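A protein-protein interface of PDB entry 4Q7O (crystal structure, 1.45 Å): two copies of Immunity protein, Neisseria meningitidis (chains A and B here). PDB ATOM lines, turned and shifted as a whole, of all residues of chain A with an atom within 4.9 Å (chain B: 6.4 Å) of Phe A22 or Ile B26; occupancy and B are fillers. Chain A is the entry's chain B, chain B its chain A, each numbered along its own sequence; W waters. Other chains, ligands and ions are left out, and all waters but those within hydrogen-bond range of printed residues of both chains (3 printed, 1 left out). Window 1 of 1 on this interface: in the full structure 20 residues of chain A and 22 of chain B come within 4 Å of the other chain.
Asn A13 touches Phe B22, but with the chains exchanged Phe A22 does not touch Asn B13 (8.5 Å). Phe A22 touches Ile B26, but with the chains exchanged Ile A26 does not touch Phe B22 (7.9 Å). Ser A25 touches Ile B26, but with the chains exchanged Ile A26 does not touch Ser B25 (8.5 Å). Ser A25 touches Glu B98, but with the chains exchanged Glu A98 does not touch Ser B25 (9.7 Å). Positions printed for both chains: 13, 16, 21, 22, 23, 24, 25, 26 and 98.
Among the printed residues, pairs that only touch across the chains: Asn A13 with Phe B22 (3.5 Å), Ile A17 with Asn B13 (3.7 Å), Ile A17 with Phe B22 (3.8 Å), Ile A17 with Ser B25 (3.6 Å), Asn A20 with Met B4 (3.2 Å), Asn A20 with Glu B29 (3.4 Å), Phe A22 with Ile B26 (3.97 Å), Phe A22 with Glu B29 (3.5 Å), Phe A22 with Thr B30 (3.5 Å), Phe A22 with Phe B34 (3.6 Å), Ser A25 with Ile B26 (3.7 Å), Ser A25 with Glu B98 (3.996 Å), Ile A26 with Ile B26 (3.6 Å), Ile A26 with Glu B98 (3.5 Å), Glu A98 with Thr B30 (3.9 Å), Glu A98 with Phe B34 (3.6 Å), Glu A98 with Gly B57 (3.3 Å) and Glu A98 with Gly B92 (3.5 Å).
Phe A22 touches just these residues of chain B: Ile B26 (3.97 Å), Glu B29 (3.5 Å), Thr B30 (3.5 Å) and Phe B34 (3.6 Å). Ile B26 touches three residues of chain A. Printed residues of chain B within 4 Å of Ile A26: Ile B26 (3.6 Å) and Glu B98 (3.5 Å). Printed residues of chain B within 4 Å of Ser A25: Ile B26 (3.7 Å) and Glu B98 (3.996 Å). His B21 touches none of the printed residues of chain A. Ser A16 touches none of the printed residues of chain B. The nearest residue of chain A that does not touch Ile B26 is Asn A13 (4.02 Å). The nearest printed residue of chain B that does not touch Ile A17 is Ile B26 (4.2 Å).
OG of Ser B25 lies within hydrogen-bond range of OD1 of Asn B13, at 2.6 Å. OE2 of Glu B29 is in hydrogen-bond range of ND2 of Asn B13, 3.1 Å away. The backbone NH of Glu B98 is in hydrogen-bond range of the backbone carbonyl oxygen of Val B91 (2.9 Å). The side-chain hydroxyl of Ser A16 sits at hydrogen-bond distance from the backbone carbonyl oxygen of Asn A13 (3.4 Å). The side-chain hydroxyl (OG) of Ser A25 lies within hydrogen-bond range of the side-chain hydroxyl (OG) of Ser A16 (2.8 Å). The backbone carbonyl oxygen of Phe A22 lies close to the side-chain hydroxyl of Ser A25 (3.4 Å).
Printed residues of chain B that touch a printed residue of chain A: Met B4, Asn B13, Phe B22, Ser B25, Ile B26, Glu B29, Thr B30, Gln B33, Phe B34, Gly B57, Gly B92 and Glu B98. Hydrophobic or aromatic side chains of chain B that line the printed part of chain A: Met B4, Phe B22, Ile B26 and Phe B34. Hydrophobic or aromatic side chains of chain A that line the printed part of chain B: Ile A17, Phe A22 and Ile A26. Along chain A the printed residues that touch a printed residue of chain B span positions 13 to 98. Among the printed residues, no Asp or Glu carboxylate lies within 4 Å of a Lys or Arg side-chain nitrogen of the other chain.
The side-chain carboxylate of Glu B29 sits close to the backbone carbonyl oxygen of Ile A17, at 2.7 Å. The side-chain amide nitrogen (NE2) of Gln B33 lies close to the side-chain amide nitrogen (ND2) of Asn A20 (3.4 Å).
Water W3 lies within hydrogen-bond range of OE1 of Glu A98 (2.5 Å), OG1 of Thr B30 (2.7 Å) and O of Gly B57 (2.7 Å). Water W1 lies within hydrogen-bond range of the side-chain amide oxygen (OD1) of Asn A20 (2.7 Å), the backbone carbonyl oxygen (O) of Glu B29 (2.9 Å) and the side-chain amide nitrogen (NE2) of Gln B33 (3.1 Å). Water W2 lies within hydrogen-bond range of OE2 of Glu A98 (2.8 Å) and O of Gly B92 (3.5 Å).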
ATOM      1  N   ASN A  13      15.837  -9.897 -15.856  1.00  0.00           N
ATOM      2  CA  ASN A  13      15.888 -10.678 -14.631  1.00  0.00           C
ATOM      3  C   ASN A  13      14.536 -10.758 -13.956  1.00  0.00           C
ATOM      4  O   ASN A  13      14.146 -11.812 -13.473  1.00  0.00           O
ATOM      5  CB  ASN A  13      16.920 -10.105 -13.648  1.00  0.00           C
ATOM      6  CG  ASN A  13      18.309 -10.659 -13.870  1.00  0.00           C
ATOM      7  OD1 ASN A  13      18.584 -11.823 -13.551  1.00  0.00           O
ATOM      8  ND2 ASN A  13      19.205  -9.825 -14.381  1.00  0.00           N
ATOM      9  N   SER A  16      12.327 -13.215 -16.109  1.00  0.00           N
ATOM     10  CA  SER A  16      12.809 -14.584 -16.113  1.00  0.00           C
ATOM     11  C   SER A  16      12.734 -15.234 -14.723  1.00  0.00           C
ATOM     12  O   SER A  16      12.317 -16.386 -14.600  1.00  0.00           O
ATOM     13  CB  SER A  16      14.213 -14.673 -16.723  1.00  0.00           C
ATOM     14  OG  SER A  16      15.141 -13.895 -15.990  1.00  0.00           O
ATOM     15  N   ILE A  17      13.125 -14.502 -13.684  1.00  0.00           N
ATOM     16  CA  ILE A  17      13.029 -15.019 -12.324  1.00  0.00           C
ATOM     17  C   ILE A  17      11.577 -15.297 -11.949  1.00  0.00           C
ATOM     18  O   ILE A  17      11.261 -16.349 -11.388  1.00  0.00           O
ATOM     19  CB  ILE A  17      13.704 -14.067 -11.306  1.00  0.00           C
ATOM     20  CG1 ILE A  17      15.220 -14.095 -11.508  1.00  0.00           C
ATOM     21  CG2 ILE A  17      13.338 -14.436  -9.867  1.00  0.00           C
ATOM     22  CD1 ILE A  17      15.937 -12.975 -10.792  1.00  0.00           C
ATOM     23  N   ASN A  20      10.451 -18.526 -13.285  1.00  0.00           N
ATOM     24  CA  ASN A  20      11.254 -19.686 -12.876  1.00  0.00           C
ATOM     25  C   ASN A  20      12.221 -20.106 -13.990  1.00  0.00           C
ATOM     26  O   ASN A  20      12.639 -21.257 -14.075  1.00  0.00           O
ATOM     27  CB  ASN A  20      10.359 -20.857 -12.441  1.00  0.00           C
ATOM     28  CG  ASN A  20      11.029 -21.784 -11.441  1.00  0.00           C
ATOM     29  OD1 ASN A  20      12.026 -21.434 -10.802  1.00  0.00           O
ATOM     30  ND2 ASN A  20      10.466 -22.980 -11.292  1.00  0.00           N
ATOM     31  N   HIS A  21      12.583 -19.153 -14.842  1.00  0.00           N
ATOM     32  CA  HIS A  21      13.522 -19.414 -15.936  1.00  0.00           C
ATOM     33  C   HIS A  21      14.879 -18.791 -15.659  1.00  0.00           C
ATOM     34  O   HIS A  21      15.412 -18.029 -16.472  1.00  0.00           O
ATOM     35  CB  HIS A  21      12.937 -18.916 -17.257  1.00  0.00           C
ATOM     36  CG  HIS A  21      11.718 -19.676 -17.673  1.00  0.00           C
ATOM     37  ND1 HIS A  21      10.777 -19.166 -18.543  1.00  0.00           N
ATOM     38  CD2 HIS A  21      11.286 -20.916 -17.339  1.00  0.00           C
ATOM     39  CE1 HIS A  21       9.823 -20.058 -18.723  1.00  0.00           C
ATOM     40  NE2 HIS A  21      10.109 -21.132 -18.006  1.00  0.00           N
ATOM     41  N   PHE A  22      15.422 -19.131 -14.495  1.00  0.00           N
ATOM     42  CA  PHE A  22      16.695 -18.598 -14.035  1.00  0.00           C
ATOM     43  C   PHE A  22      17.861 -18.919 -14.974  1.00  0.00           C
ATOM     44  O   PHE A  22      18.846 -18.188 -15.003  1.00  0.00           O
ATOM     45  CB  PHE A  22      16.994 -19.083 -12.613  1.00  0.00           C
ATOM     46  CG  PHE A  22      16.945 -20.578 -12.465  1.00  0.00           C
ATOM     47  CD1 PHE A  22      18.079 -21.351 -12.691  1.00  0.00           C
ATOM     48  CD2 PHE A  22      15.762 -21.213 -12.106  1.00  0.00           C
ATOM     49  CE1 PHE A  22      18.043 -22.730 -12.552  1.00  0.00           C
ATOM     50  CE2 PHE A  22      15.711 -22.594 -11.973  1.00  0.00           C
ATOM     51  CZ  PHE A  22      16.855 -23.359 -12.200  1.00  0.00           C
ATOM     52  N   VAL A  23      17.751 -19.985 -15.763  1.00  0.00           N
ATOM     53  CA  VAL A  23      18.790 -20.281 -16.753  1.00  0.00           C
ATOM     54  C   VAL A  23      18.963 -19.124 -17.745  1.00  0.00           C
ATOM     55  O   VAL A  23      20.093 -18.793 -18.142  1.00  0.00           O
ATOM     56  CB  VAL A  23      18.501 -21.621 -17.483  1.00  0.00           C
ATOM     57  CG1 VAL A  23      19.317 -21.738 -18.767  1.00  0.00           C
ATOM     58  CG2 VAL A  23      18.792 -22.802 -16.554  1.00  0.00           C
ATOM     59  N   ILE A  24      17.848 -18.498 -18.124  1.00  0.00           N
ATOM     60  CA  ILE A  24      17.897 -17.342 -19.018  1.00  0.00           C
ATOM     61  C   ILE A  24      18.628 -16.157 -18.381  1.00  0.00           C
ATOM     62  O   ILE A  24      19.425 -15.481 -19.041  1.00  0.00           O
ATOM     63  CB  ILE A  24      16.487 -16.900 -19.453  1.00  0.00           C
ATOM     64  CG1 ILE A  24      15.755 -18.048 -20.160  1.00  0.00           C
ATOM     65  CG2 ILE A  24      16.568 -15.670 -20.345  1.00  0.00           C
ATOM     66  CD1 ILE A  24      16.484 -18.600 -21.370  1.00  0.00           C
ATOM     67  N   SER A  25      18.344 -15.911 -17.104  1.00  0.00           N
ATOM     68  CA  SER A  25      19.004 -14.858 -16.330  1.00  0.00           C
ATOM     69  C   SER A  25      20.520 -15.063 -16.354  1.00  0.00           C
ATOM     70  O   SER A  25      21.296 -14.133 -16.610  1.00  0.00           O
ATOM     71  CB  SER A  25      18.529 -14.882 -14.865  1.00  0.00           C
ATOM     72  OG  SER A  25      17.171 -15.289 -14.728  1.00  0.00           O
ATOM     73  N   ILE A  26      20.942 -16.294 -16.087  1.00  0.00           N
ATOM     74  CA  ILE A  26      22.364 -16.613 -16.023  1.00  0.00           C
ATOM     75  C   ILE A  26      23.002 -16.513 -17.400  1.00  0.00           C
ATOM     76  O   ILE A  26      24.110 -15.999 -17.544  1.00  0.00           O
ATOM     77  CB  ILE A  26      22.580 -18.031 -15.456  1.00  0.00           C
ATOM     78  CG1 ILE A  26      22.064 -18.112 -14.018  1.00  0.00           C
ATOM     79  CG2 ILE A  26      24.053 -18.439 -15.510  1.00  0.00           C
ATOM     80  CD1 ILE A  26      22.040 -19.532 -13.486  1.00  0.00           C
ATOM     81  N   GLU A  98      23.240 -26.669 -16.578  1.00  0.00           N
ATOM     82  CA  GLU A  98      21.912 -26.282 -16.115  1.00  0.00           C
ATOM     83  C   GLU A  98      21.088 -25.978 -17.359  1.00  0.00           C
ATOM     84  O   GLU A  98      21.435 -25.090 -18.137  1.00  0.00           O
ATOM     85  CB  GLU A  98      22.010 -25.051 -15.226  1.00  0.00           C
ATOM     86  CG  GLU A  98      23.023 -25.190 -14.108  1.00  0.00           C
ATOM     87  CD  GLU A  98      23.107 -23.932 -13.270  1.00  0.00           C
ATOM     88  OE1 GLU A  98      22.038 -23.454 -12.823  1.00  0.00           O
ATOM     89  OE2 GLU A  98      24.228 -23.410 -13.076  1.00  0.00           O
ATOM     90  N   MET B   4       8.376 -28.290 -15.101  1.00  0.00           N
ATOM     91  CA  MET B   4       9.374 -28.237 -14.034  1.00  0.00           C
ATOM     92  C   MET B   4       8.696 -28.049 -12.678  1.00  0.00           C
ATOM     93  O   MET B   4       7.468 -27.927 -12.613  1.00  0.00           O
ATOM     94  CB  MET B   4      10.396 -27.123 -14.317  1.00  0.00           C
ATOM     95  CG  MET B   4       9.799 -25.739 -14.550  1.00  0.00           C
ATOM     96  SD  MET B   4      10.906 -24.584 -15.411  1.00  0.00           S
ATOM     97  CE  MET B   4      12.246 -24.426 -14.227  1.00  0.00           C
ATOM     98  N   ASN B  13      11.245 -13.569  -4.116  1.00  0.00           N
ATOM     99  CA  ASN B  13      11.422 -12.957  -5.432  1.00  0.00           C
ATOM    100  C   ASN B  13      11.011 -11.490  -5.466  1.00  0.00           C
ATOM    101  O   ASN B  13      11.681 -10.677  -6.090  1.00  0.00           O
ATOM    102  CB  ASN B  13      10.696 -13.751  -6.525  1.00  0.00           C
ATOM    103  CG  ASN B  13      11.372 -15.070  -6.831  1.00  0.00           C
ATOM    104  OD1 ASN B  13      12.492 -15.314  -6.398  1.00  0.00           O
ATOM    105  ND2 ASN B  13      10.690 -15.930  -7.584  1.00  0.00           N
ATOM    106  N   SER B  16      14.004  -9.626  -3.528  1.00  0.00           N
ATOM    107  CA  SER B  16      15.292  -9.650  -4.212  1.00  0.00           C
ATOM    108  C   SER B  16      15.241  -8.833  -5.512  1.00  0.00           C
ATOM    109  O   SER B  16      16.192  -8.119  -5.847  1.00  0.00           O
ATOM    110  CB  SER B  16      15.709 -11.086  -4.501  1.00  0.00           C
ATOM    111  OG  SER B  16      14.892 -11.614  -5.525  1.00  0.00           O
ATOM    112  N   HIS B  21      18.938  -7.663  -6.385  1.00  0.00           N
ATOM    113  CA  HIS B  21      19.811  -8.753  -5.953  1.00  0.00           C
ATOM    114  C   HIS B  21      19.348 -10.058  -6.574  1.00  0.00           C
ATOM    115  O   HIS B  21      18.976 -11.027  -5.884  1.00  0.00           O
ATOM    116  CB  HIS B  21      19.853  -8.837  -4.426  1.00  0.00           C
ATOM    117  CG  HIS B  21      20.598  -7.703  -3.796  1.00  0.00           C
ATOM    118  ND1 HIS B  21      20.359  -7.269  -2.511  1.00  0.00           N
ATOM    119  CD2 HIS B  21      21.570  -6.902  -4.293  1.00  0.00           C
ATOM    120  CE1 HIS B  21      21.162  -6.251  -2.240  1.00  0.00           C
ATOM    121  NE2 HIS B  21      21.908  -6.011  -3.305  1.00  0.00           N
ATOM    122  N   PHE B  22      19.370 -10.060  -7.897  1.00  0.00           N
ATOM    123  CA  PHE B  22      18.862 -11.172  -8.679  1.00  0.00           C
ATOM    124  C   PHE B  22      19.528 -12.502  -8.362  1.00  0.00           C
ATOM    125  O   PHE B  22      18.872 -13.548  -8.376  1.00  0.00           O
ATOM    126  CB  PHE B  22      18.972 -10.835 -10.161  1.00  0.00           C
ATOM    127  CG  PHE B  22      18.380  -9.503 -10.504  1.00  0.00           C
ATOM    128  CD1 PHE B  22      17.041  -9.249 -10.262  1.00  0.00           C
ATOM    129  CD2 PHE B  22      19.154  -8.502 -11.060  1.00  0.00           C
ATOM    130  CE1 PHE B  22      16.486  -8.021 -10.567  1.00  0.00           C
ATOM    131  CE2 PHE B  22      18.606  -7.271 -11.367  1.00  0.00           C
ATOM    132  CZ  PHE B  22      17.268  -7.033 -11.119  1.00  0.00           C
ATOM    133  N   VAL B  23      20.825 -12.465  -8.061  1.00  0.00           N
ATOM    134  CA  VAL B  23      21.557 -13.682  -7.736  1.00  0.00           C
ATOM    135  C   VAL B  23      20.933 -14.453  -6.560  1.00  0.00           C
ATOM    136  O   VAL B  23      20.947 -15.684  -6.547  1.00  0.00           O
ATOM    137  CB  VAL B  23      23.055 -13.366  -7.485  1.00  0.00           C
ATOM    138  CG1 VAL B  23      23.758 -14.501  -6.743  1.00  0.00           C
ATOM    139  CG2 VAL B  23      23.746 -13.062  -8.809  1.00  0.00           C
ATOM    140  N   ILE B  24      20.356 -13.743  -5.593  1.00  0.00           N
ATOM    141  CA  ILE B  24      19.738 -14.423  -4.462  1.00  0.00           C
ATOM    142  C   ILE B  24      18.550 -15.291  -4.913  1.00  0.00           C
ATOM    143  O   ILE B  24      18.420 -16.448  -4.504  1.00  0.00           O
ATOM    144  CB  ILE B  24      19.308 -13.434  -3.358  1.00  0.00           C
ATOM    145  CG1 ILE B  24      20.518 -12.620  -2.869  1.00  0.00           C
ATOM    146  CG2 ILE B  24      18.672 -14.176  -2.191  1.00  0.00           C
ATOM    147  CD1 ILE B  24      21.706 -13.458  -2.363  1.00  0.00           C
ATOM    148  N   SER B  25      17.687 -14.746  -5.762  1.00  0.00           N
ATOM    149  CA  SER B  25      16.587 -15.542  -6.296  1.00  0.00           C
ATOM    150  C   SER B  25      17.057 -16.654  -7.221  1.00  0.00           C
ATOM    151  O   SER B  25      16.529 -17.759  -7.176  1.00  0.00           O
ATOM    152  CB  SER B  25      15.566 -14.666  -7.001  1.00  0.00           C
ATOM    153  OG  SER B  25      14.716 -14.064  -6.036  1.00  0.00           O
ATOM    154  N   ILE B  26      18.050 -16.376  -8.058  1.00  0.00           N
ATOM    155  CA  ILE B  26      18.577 -17.423  -8.929  1.00  0.00           C
ATOM    156  C   ILE B  26      19.134 -18.571  -8.084  1.00  0.00           C
ATOM    157  O   ILE B  26      18.901 -19.751  -8.381  1.00  0.00           O
ATOM    158  CB  ILE B  26      19.645 -16.880  -9.886  1.00  0.00           C
ATOM    159  CG1 ILE B  26      19.015 -15.855 -10.829  1.00  0.00           C
ATOM    160  CG2 ILE B  26      20.292 -18.022 -10.678  1.00  0.00           C
ATOM    161  CD1 ILE B  26      20.027 -14.976 -11.510  1.00  0.00           C
ATOM    162  N   PHE B  27      19.842 -18.212  -7.017  1.00  0.00           N
ATOM    163  CA  PHE B  27      20.422 -19.170  -6.088  1.00  0.00           C
ATOM    164  C   PHE B  27      19.339 -20.106  -5.534  1.00  0.00           C
ATOM    165  O   PHE B  27      19.448 -21.338  -5.631  1.00  0.00           O
ATOM    166  CB  PHE B  27      21.138 -18.403  -4.968  1.00  0.00           C
ATOM    167  CG  PHE B  27      21.634 -19.266  -3.840  1.00  0.00           C
ATOM    168  CD1 PHE B  27      22.909 -19.819  -3.869  1.00  0.00           C
ATOM    169  CD2 PHE B  27      20.829 -19.509  -2.731  1.00  0.00           C
ATOM    170  CE1 PHE B  27      23.363 -20.607  -2.811  1.00  0.00           C
ATOM    171  CE2 PHE B  27      21.274 -20.295  -1.683  1.00  0.00           C
ATOM    172  CZ  PHE B  27      22.539 -20.848  -1.722  1.00  0.00           C
ATOM    173  N   PHE B  28      18.286 -19.536  -4.960  1.00  0.00           N
ATOM    174  CA  PHE B  28      17.235 -20.364  -4.378  1.00  0.00           C
ATOM    175  C   PHE B  28      16.434 -21.156  -5.415  1.00  0.00           C
ATOM    176  O   PHE B  28      16.123 -22.331  -5.193  1.00  0.00           O
ATOM    177  CB  PHE B  28      16.328 -19.545  -3.449  1.00  0.00           C
ATOM    178  CG  PHE B  28      16.917 -19.348  -2.081  1.00  0.00           C
ATOM    179  CD1 PHE B  28      17.044 -20.428  -1.217  1.00  0.00           C
ATOM    180  CD2 PHE B  28      17.396 -18.108  -1.679  1.00  0.00           C
ATOM    181  CE1 PHE B  28      17.606 -20.277   0.038  1.00  0.00           C
ATOM    182  CE2 PHE B  28      17.958 -17.936  -0.413  1.00  0.00           C
ATOM    183  CZ  PHE B  28      18.066 -19.026   0.447  1.00  0.00           C
ATOM    184  N   GLU B  29      16.118 -20.540  -6.549  1.00  0.00           N
ATOM    185  CA  GLU B  29      15.389 -21.251  -7.600  1.00  0.00           C
ATOM    186  C   GLU B  29      16.181 -22.452  -8.118  1.00  0.00           C
ATOM    187  O   GLU B  29      15.612 -23.508  -8.404  1.00  0.00           O
ATOM    188  CB  GLU B  29      15.012 -20.311  -8.755  1.00  0.00           C
ATOM    189  CG  GLU B  29      13.863 -19.351  -8.420  1.00  0.00           C
ATOM    190  CD  GLU B  29      13.373 -18.507  -9.595  1.00  0.00           C
ATOM    191  OE1 GLU B  29      14.037 -18.471 -10.656  1.00  0.00           O
ATOM    192  OE2 GLU B  29      12.309 -17.863  -9.437  1.00  0.00           O
ATOM    193  N   THR B  30      17.495 -22.278  -8.219  1.00  0.00           N
ATOM    194  CA  THR B  30      18.392 -23.338  -8.667  1.00  0.00           C
ATOM    195  C   THR B  30      18.354 -24.532  -7.716  1.00  0.00           C
ATOM    196  O   THR B  30      18.166 -25.670  -8.138  1.00  0.00           O
ATOM    197  CB  THR B  30      19.846 -22.829  -8.767  1.00  0.00           C
ATOM    198  OG1 THR B  30      19.935 -21.813  -9.775  1.00  0.00           O
ATOM    199  CG2 THR B  30      20.797 -23.960  -9.116  1.00  0.00           C
ATOM    200  N   ILE B  31      18.550 -24.271  -6.428  1.00  0.00           N
ATOM    201  CA  ILE B  31      18.606 -25.352  -5.455  1.00  0.00           C
ATOM    202  C   ILE B  31      17.265 -26.069  -5.365  1.00  0.00           C
ATOM    203  O   ILE B  31      17.216 -27.297  -5.334  1.00  0.00           O
ATOM    204  CB  ILE B  31      19.075 -24.848  -4.073  1.00  0.00           C
ATOM    205  CG1 ILE B  31      20.520 -24.359  -4.184  1.00  0.00           C
ATOM    206  CG2 ILE B  31      18.956 -25.945  -3.022  1.00  0.00           C
ATOM    207  CD1 ILE B  31      20.971 -23.520  -3.030  1.00  0.00           C
ATOM    208  N   GLN B  33      14.975 -26.332  -7.665  1.00  0.00           N
ATOM    209  CA  GLN B  33      14.688 -27.084  -8.879  1.00  0.00           C
ATOM    210  C   GLN B  33      15.538 -28.354  -9.000  1.00  0.00           C
ATOM    211  O   GLN B  33      15.031 -29.413  -9.365  1.00  0.00           O
ATOM    212  CB  GLN B  33      14.917 -26.209 -10.115  1.00  0.00           C
ATOM    213  CG  GLN B  33      14.321 -26.803 -11.379  1.00  0.00           C
ATOM    214  CD  GLN B  33      12.800 -26.870 -11.316  1.00  0.00           C
ATOM    215  OE1 GLN B  33      12.199 -27.830 -11.789  1.00  0.00           O
ATOM    216  NE2 GLN B  33      12.176 -25.847 -10.730  1.00  0.00           N
ATOM    217  N   PHE B  34      16.831 -28.247  -8.709  1.00  0.00           N
ATOM    218  CA  PHE B  34      17.761 -29.329  -9.037  1.00  0.00           C
ATOM    219  C   PHE B  34      18.098 -30.270  -7.879  1.00  0.00           C
ATOM    220  O   PHE B  34      18.615 -31.363  -8.102  1.00  0.00           O
ATOM    221  CB  PHE B  34      19.070 -28.770  -9.614  1.00  0.00           C
ATOM    222  CG  PHE B  34      18.901 -27.946 -10.855  1.00  0.00           C
ATOM    223  CD1 PHE B  34      17.898 -28.217 -11.774  1.00  0.00           C
ATOM    224  CD2 PHE B  34      19.766 -26.893 -11.106  1.00  0.00           C
ATOM    225  CE1 PHE B  34      17.756 -27.436 -12.921  1.00  0.00           C
ATOM    226  CE2 PHE B  34      19.637 -26.123 -12.250  1.00  0.00           C
ATOM    227  CZ  PHE B  34      18.629 -26.394 -13.153  1.00  0.00           C
ATOM    228  N   GLY B  57      26.122 -25.125  -9.671  1.00  0.00           N
ATOM    229  CA  GLY B  57      25.334 -23.975 -10.069  1.00  0.00           C
ATOM    230  C   GLY B  57      24.940 -22.969  -9.000  1.00  0.00           C
ATOM    231  O   GLY B  57      24.369 -21.932  -9.335  1.00  0.00           O
ATOM    232  N   ALA B  58      25.245 -23.229  -7.729  1.00  0.00           N
ATOM    233  CA  ALA B  58      24.865 -22.285  -6.678  1.00  0.00           C
ATOM    234  C   ALA B  58      25.683 -22.491  -5.411  1.00  0.00           C
ATOM    235  O   ALA B  58      25.776 -23.604  -4.900  1.00  0.00           O
ATOM    236  CB  ALA B  58      23.377 -22.423  -6.363  1.00  0.00           C
ATOM    237  N   VAL B  91      26.279 -18.044  -8.749  1.00  0.00           N
ATOM    238  CA  VAL B  91      25.469 -18.985  -9.498  1.00  0.00           C
ATOM    239  C   VAL B  91      26.106 -19.199 -10.865  1.00  0.00           C
ATOM    240  O   VAL B  91      26.922 -18.394 -11.310  1.00  0.00           O
ATOM    241  CB  VAL B  91      24.006 -18.516  -9.621  1.00  0.00           C
ATOM    242  CG1 VAL B  91      23.343 -18.507  -8.255  1.00  0.00           C
ATOM    243  CG2 VAL B  91      23.932 -17.145 -10.287  1.00  0.00           C
ATOM    244  N   GLY B  92      25.763 -20.301 -11.520  1.00  0.00           N
ATOM    245  CA  GLY B  92      26.469 -20.693 -12.728  1.00  0.00           C
ATOM    246  C   GLY B  92      27.724 -21.491 -12.390  1.00  0.00           C
ATOM    247  O   GLY B  92      27.838 -22.032 -11.288  1.00  0.00           O
ATOM    248  N   GLU B  98      28.240 -15.952 -12.053  1.00  0.00           N
ATOM    249  CA  GLU B  98      27.514 -14.727 -11.770  1.00  0.00           C
ATOM    250  C   GLU B  98      27.588 -14.525 -10.258  1.00  0.00           C
ATOM    251  O   GLU B  98      27.223 -15.417  -9.494  1.00  0.00           O
ATOM    252  CB  GLU B  98      26.073 -14.860 -12.261  1.00  0.00           C
ATOM    253  CG  GLU B  98      25.237 -13.647 -11.978  1.00  0.00           C
ATOM    254  CD  GLU B  98      23.874 -13.690 -12.650  1.00  0.00           C
ATOM    255  OE1 GLU B  98      23.572 -14.668 -13.369  1.00  0.00           O
ATOM    256  OE2 GLU B  98      23.101 -12.737 -12.458  1.00  0.00           O
HETATM  257  O   HOH W   1      12.828 -23.322  -9.000  1.00  0.00           O
HETATM  258  O   HOH W   2      26.807 -24.521 -13.456  1.00  0.00           O
HETATM  259  O   HOH W   3      22.302 -21.618 -11.102  1.00  0.00           O
